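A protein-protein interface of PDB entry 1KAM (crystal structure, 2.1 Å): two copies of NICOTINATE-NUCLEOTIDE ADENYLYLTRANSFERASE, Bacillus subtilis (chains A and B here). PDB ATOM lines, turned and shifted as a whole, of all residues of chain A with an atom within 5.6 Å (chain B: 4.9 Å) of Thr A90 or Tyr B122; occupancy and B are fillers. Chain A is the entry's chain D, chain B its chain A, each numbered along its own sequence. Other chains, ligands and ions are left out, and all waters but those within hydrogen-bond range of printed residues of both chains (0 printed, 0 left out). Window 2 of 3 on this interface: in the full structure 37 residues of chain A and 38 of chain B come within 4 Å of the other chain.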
ATOM      1  N   ARG A  84      33.812  24.754 -17.990  1.00  0.00           N
ATOM      2  CA  ARG A  84      32.668  25.235 -18.758  1.00  0.00           C
ATOM      3  C   ARG A  84      33.029  26.352 -19.737  1.00  0.00           C
ATOM      4  O   ARG A  84      32.258  26.650 -20.651  1.00  0.00           O
ATOM      5  CB  ARG A  84      31.559  25.727 -17.826  1.00  0.00           C
ATOM      6  CG  ARG A  84      30.950  24.670 -16.928  1.00  0.00           C
ATOM      7  CD  ARG A  84      29.810  25.260 -16.106  1.00  0.00           C
ATOM      8  NE  ARG A  84      30.210  26.478 -15.401  1.00  0.00           N
ATOM      9  CZ  ARG A  84      29.652  27.673 -15.585  1.00  0.00           C
ATOM     10  NH1 ARG A  84      28.662  27.826 -16.453  1.00  0.00           N
ATOM     11  NH2 ARG A  84      30.085  28.722 -14.898  1.00  0.00           N
ATOM     12  N   GLU A  85      34.187  26.978 -19.543  1.00  0.00           N
ATOM     13  CA  GLU A  85      34.621  28.047 -20.437  1.00  0.00           C
ATOM     14  C   GLU A  85      35.503  27.548 -21.572  1.00  0.00           C
ATOM     15  O   GLU A  85      36.571  26.985 -21.340  1.00  0.00           O
ATOM     16  CB  GLU A  85      35.381  29.133 -19.673  1.00  0.00           C
ATOM     17  CG  GLU A  85      34.510  30.248 -19.122  1.00  0.00           C
ATOM     18  CD  GLU A  85      35.294  31.532 -18.910  1.00  0.00           C
ATOM     19  OE1 GLU A  85      35.673  32.172 -19.916  1.00  0.00           O
ATOM     20  OE2 GLU A  85      35.539  31.896 -17.741  1.00  0.00           O
ATOM     21  N   GLY A  86      35.044  27.764 -22.802  1.00  0.00           N
ATOM     22  CA  GLY A  86      35.805  27.364 -23.973  1.00  0.00           C
ATOM     23  C   GLY A  86      36.146  28.630 -24.745  1.00  0.00           C
ATOM     24  O   GLY A  86      36.261  28.607 -25.974  1.00  0.00           O
ATOM     25  N   SER A  88      34.874  31.377 -25.948  1.00  0.00           N
ATOM     26  CA  SER A  88      33.975  32.098 -26.851  1.00  0.00           C
ATOM     27  C   SER A  88      32.547  31.813 -26.411  1.00  0.00           C
ATOM     28  O   SER A  88      31.628  32.614 -26.624  1.00  0.00           O
ATOM     29  CB  SER A  88      34.162  31.637 -28.295  1.00  0.00           C
ATOM     30  OG  SER A  88      35.319  32.217 -28.873  1.00  0.00           O
ATOM     31  N   TYR A  89      32.379  30.654 -25.787  1.00  0.00           N
ATOM     32  CA  TYR A  89      31.081  30.230 -25.299  1.00  0.00           C
ATOM     33  C   TYR A  89      31.247  29.510 -23.968  1.00  0.00           C
ATOM     34  O   TYR A  89      32.165  28.711 -23.795  1.00  0.00           O
ATOM     35  CB  TYR A  89      30.412  29.289 -26.304  1.00  0.00           C
ATOM     36  CG  TYR A  89      29.063  28.802 -25.838  1.00  0.00           C
ATOM     37  CD1 TYR A  89      27.985  29.683 -25.732  1.00  0.00           C
ATOM     38  CD2 TYR A  89      28.878  27.477 -25.441  1.00  0.00           C
ATOM     39  CE1 TYR A  89      26.759  29.260 -25.235  1.00  0.00           C
ATOM     40  CE2 TYR A  89      27.655  27.041 -24.941  1.00  0.00           C
ATOM     41  CZ  TYR A  89      26.601  27.940 -24.838  1.00  0.00           C
ATOM     42  OH  TYR A  89      25.402  27.536 -24.311  1.00  0.00           O
ATOM     43  N   THR A  90      30.360  29.798 -23.030  1.00  0.00           N
ATOM     44  CA  THR A  90      30.408  29.147 -21.728  1.00  0.00           C
ATOM     45  C   THR A  90      29.186  28.242 -21.581  1.00  0.00           C
ATOM     46  O   THR A  90      28.051  28.699 -21.710  1.00  0.00           O
ATOM     47  CB  THR A  90      30.431  30.192 -20.581  1.00  0.00           C
ATOM     48  OG1 THR A  90      31.645  30.950 -20.650  1.00  0.00           O
ATOM     49  CG2 THR A  90      30.356  29.504 -19.224  1.00  0.00           C
ATOM     50  N   PHE A  91      29.433  26.955 -21.357  1.00  0.00           N
ATOM     51  CA  PHE A  91      28.370  25.966 -21.169  1.00  0.00           C
ATOM     52  C   PHE A  91      27.979  25.973 -19.697  1.00  0.00           C
ATOM     53  O   PHE A  91      28.744  26.415 -18.844  1.00  0.00           O
ATOM     54  CB  PHE A  91      28.873  24.544 -21.435  1.00  0.00           C
ATOM     55  CG  PHE A  91      29.013  24.171 -22.881  1.00  0.00           C
ATOM     56  CD1 PHE A  91      28.013  23.435 -23.522  1.00  0.00           C
ATOM     57  CD2 PHE A  91      30.176  24.471 -23.582  1.00  0.00           C
ATOM     58  CE1 PHE A  91      28.173  22.999 -24.832  1.00  0.00           C
ATOM     59  CE2 PHE A  91      30.344  24.035 -24.903  1.00  0.00           C
ATOM     60  CZ  PHE A  91      29.342  23.299 -25.525  1.00  0.00           C
ATOM     61  N   ASP A  92      26.784  25.488 -19.393  1.00  0.00           N
ATOM     62  CA  ASP A  92      26.426  25.357 -17.997  1.00  0.00           C
ATOM     63  C   ASP A  92      26.845  23.908 -17.771  1.00  0.00           C
ATOM     64  O   ASP A  92      27.143  23.196 -18.738  1.00  0.00           O
ATOM     65  CB  ASP A  92      24.930  25.582 -17.752  1.00  0.00           C
ATOM     66  CG  ASP A  92      24.040  24.652 -18.551  1.00  0.00           C
ATOM     67  OD1 ASP A  92      22.814  24.864 -18.497  1.00  0.00           O
ATOM     68  OD2 ASP A  92      24.537  23.724 -19.221  1.00  0.00           O
ATOM     69  N   LYS B 120      25.705  24.035 -11.930  1.00  0.00           N
ATOM     70  CA  LYS B 120      25.296  25.175 -12.751  1.00  0.00           C
ATOM     71  C   LYS B 120      24.321  24.721 -13.832  1.00  0.00           C
ATOM     72  O   LYS B 120      24.604  23.776 -14.574  1.00  0.00           O
ATOM     73  CB  LYS B 120      26.517  25.833 -13.399  1.00  0.00           C
ATOM     74  CG  LYS B 120      26.193  27.134 -14.126  1.00  0.00           C
ATOM     75  CD  LYS B 120      25.559  28.138 -13.170  1.00  0.00           C
ATOM     76  CE  LYS B 120      25.393  29.499 -13.820  1.00  0.00           C
ATOM     77  NZ  LYS B 120      24.783  30.480 -12.872  1.00  0.00           N
ATOM     78  N   TRP B 121      23.177  25.396 -13.925  1.00  0.00           N
ATOM     79  CA  TRP B 121      22.147  25.039 -14.897  1.00  0.00           C
ATOM     80  C   TRP B 121      21.369  26.275 -15.345  1.00  0.00           C
ATOM     81  O   TRP B 121      20.700  26.908 -14.536  1.00  0.00           O
ATOM     82  CB  TRP B 121      21.190  24.040 -14.252  1.00  0.00           C
ATOM     83  CG  TRP B 121      20.325  23.318 -15.218  1.00  0.00           C
ATOM     84  CD1 TRP B 121      20.334  23.430 -16.579  1.00  0.00           C
ATOM     85  CD2 TRP B 121      19.366  22.311 -14.902  1.00  0.00           C
ATOM     86  NE1 TRP B 121      19.441  22.548 -17.131  1.00  0.00           N
ATOM     87  CE2 TRP B 121      18.831  21.847 -16.123  1.00  0.00           C
ATOM     88  CE3 TRP B 121      18.905  21.751 -13.703  1.00  0.00           C
ATOM     89  CZ2 TRP B 121      17.859  20.846 -16.183  1.00  0.00           C
ATOM     90  CZ3 TRP B 121      17.938  20.757 -13.761  1.00  0.00           C
ATOM     91  CH2 TRP B 121      17.425  20.313 -14.996  1.00  0.00           C
ATOM     92  N   TYR B 122      21.436  26.607 -16.633  1.00  0.00           N
ATOM     93  CA  TYR B 122      20.751  27.796 -17.138  1.00  0.00           C
ATOM     94  C   TYR B 122      19.234  27.734 -17.096  1.00  0.00           C
ATOM     95  O   TYR B 122      18.573  28.772 -17.042  1.00  0.00           O
ATOM     96  CB  TYR B 122      21.194  28.126 -18.567  1.00  0.00           C
ATOM     97  CG  TYR B 122      22.663  28.477 -18.695  1.00  0.00           C
ATOM     98  CD1 TYR B 122      23.327  29.169 -17.683  1.00  0.00           C
ATOM     99  CD2 TYR B 122      23.390  28.121 -19.837  1.00  0.00           C
ATOM    100  CE1 TYR B 122      24.685  29.496 -17.802  1.00  0.00           C
ATOM    101  CE2 TYR B 122      24.747  28.447 -19.968  1.00  0.00           C
ATOM    102  CZ  TYR B 122      25.385  29.132 -18.944  1.00  0.00           C
ATOM    103  OH  TYR B 122      26.721  29.441 -19.049  1.00  0.00           O
ATOM    104  N   LYS B 123      18.674  26.532 -17.136  1.00  0.00           N
ATOM    105  CA  LYS B 123      17.227  26.405 -17.085  1.00  0.00           C
ATOM    106  C   LYS B 123      16.751  26.821 -15.697  1.00  0.00           C
ATOM    107  O   LYS B 123      15.654  27.361 -15.536  1.00  0.00           O
ATOM    108  CB  LYS B 123      16.809  24.973 -17.408  1.00  0.00           C
ATOM    109  CG  LYS B 123      16.333  24.813 -18.843  1.00  0.00           C
ATOM    110  CD  LYS B 123      16.592  23.412 -19.376  1.00  0.00           C
ATOM    111  CE  LYS B 123      18.081  23.196 -19.637  1.00  0.00           C
ATOM    112  NZ  LYS B 123      18.406  21.802 -20.056  1.00  0.00           N
ATOM    113  N   LEU B 124      17.593  26.579 -14.696  1.00  0.00           N
ATOM    114  CA  LEU B 124      17.270  26.960 -13.332  1.00  0.00           C
ATOM    115  C   LEU B 124      17.521  28.463 -13.177  1.00  0.00           C
ATOM    116  O   LEU B 124      16.704  29.183 -12.601  1.00  0.00           O
ATOM    117  CB  LEU B 124      18.137  26.182 -12.336  1.00  0.00           C
ATOM    118  CG  LEU B 124      18.038  26.677 -10.888  1.00  0.00           C
ATOM    119  CD1 LEU B 124      16.595  26.583 -10.423  1.00  0.00           C
ATOM    120  CD2 LEU B 124      18.939  25.864  -9.985  1.00  0.00           C
ATOM    121  N   ASP B 125      18.654  28.933 -13.693  1.00  0.00           N
ATOM    122  CA  ASP B 125      18.981  30.353 -13.604  1.00  0.00           C
ATOM    123  C   ASP B 125      17.853  31.170 -14.205  1.00  0.00           C
ATOM    124  O   ASP B 125      17.464  32.209 -13.667  1.00  0.00           O
ATOM    125  CB  ASP B 125      20.274  30.669 -14.360  1.00  0.00           C
ATOM    126  CG  ASP B 125      21.502  30.117 -13.673  1.00  0.00           C
ATOM    127  OD1 ASP B 125      21.420  29.765 -12.477  1.00  0.00           O
ATOM    128  OD2 ASP B 125      22.560  30.051 -14.332  1.00  0.00           O
ATOM    129  N   GLU B 126      17.333  30.679 -15.324  1.00  0.00           N
ATOM    130  CA  GLU B 126      16.253  31.345 -16.036  1.00  0.00           C
ATOM    131  C   GLU B 126      15.012  31.463 -15.163  1.00  0.00           C
ATOM    132  O   GLU B 126      14.345  32.507 -15.146  1.00  0.00           O
ATOM    133  CB  GLU B 126      15.931  30.564 -17.310  1.00  0.00           C
ATOM    134  CG  GLU B 126      14.831  31.155 -18.167  1.00  0.00           C
ATOM    135  CD  GLU B 126      14.716  30.440 -19.504  1.00  0.00           C
ATOM    136  OE1 GLU B 126      13.631  29.889 -19.804  1.00  0.00           O
ATOM    137  OE2 GLU B 126      15.720  30.427 -20.250  1.00  0.00           O
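The backbone carbonyl oxygen (O) of Thr A90 is in hydrogen-bond range of the side-chain hydroxyl (OH) of Tyr B122 (3.1 Å). The backbone NH (N) of Tyr B122 lies within hydrogen-bond range of the side-chain carboxylate (OD1) of Asp A92 (2.9 Å).
The guanidinium group (NH1) of Arg A84 lies within hydrogen-bond range of the backbone carbonyl oxygen (O) of Phe A91 (2.8 Å). The side-chain amino group of Lys B120 is in salt-bridge range of the side-chain carboxylate of Asp B125 (2.7 Å).
Arg A84 touches Lys B120. OH of Tyr B122 touches NH1 of Arg A84 (3.6 Å). Phe A91 touches Tyr B122 (O to OH, 3.6 Å). Asp A92 touches Lys B120. Asp A92 touches Trp B121 (OD1 to CD1, 3.4 Å).
Tyr B122 touches just these residues of chain A: Arg A84 (3.6 Å), Thr A90 (3.1 Å), Phe A91 (3.6 Å) and Asp A92 (2.9 Å). Of the printed residues of chain B, Asp A92 touches Lys B120, Trp B121 and Tyr B122. Of the printed residues of chain B, Arg A84 touches Lys B120 and Tyr B122. Of the printed residues of chain B, Phe A91 touches Tyr B122. Of the printed residues of chain A, Trp B121 touches Asp A92 (3.4 Å). Of the printed residues of chain A, Lys B120 touches Arg A84 and Asp A92.
Printed residues of chain B that touch a printed residue of chain A: Lys B120, Trp B121 and Tyr B122. Hydrophobic or aromatic side chains of chain B within 4 Å of the printed part of chain A: Trp B121 and Tyr B122. Of the 8 printed residues of chain A, 4 touch a printed residue of chain B. Among the printed residues, 7 pairs touch across the chains.
No position is printed for both chains. Of the 7 pairs that touch across the chains among the printed residues, none has its exchanged pair printed and touching as well.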
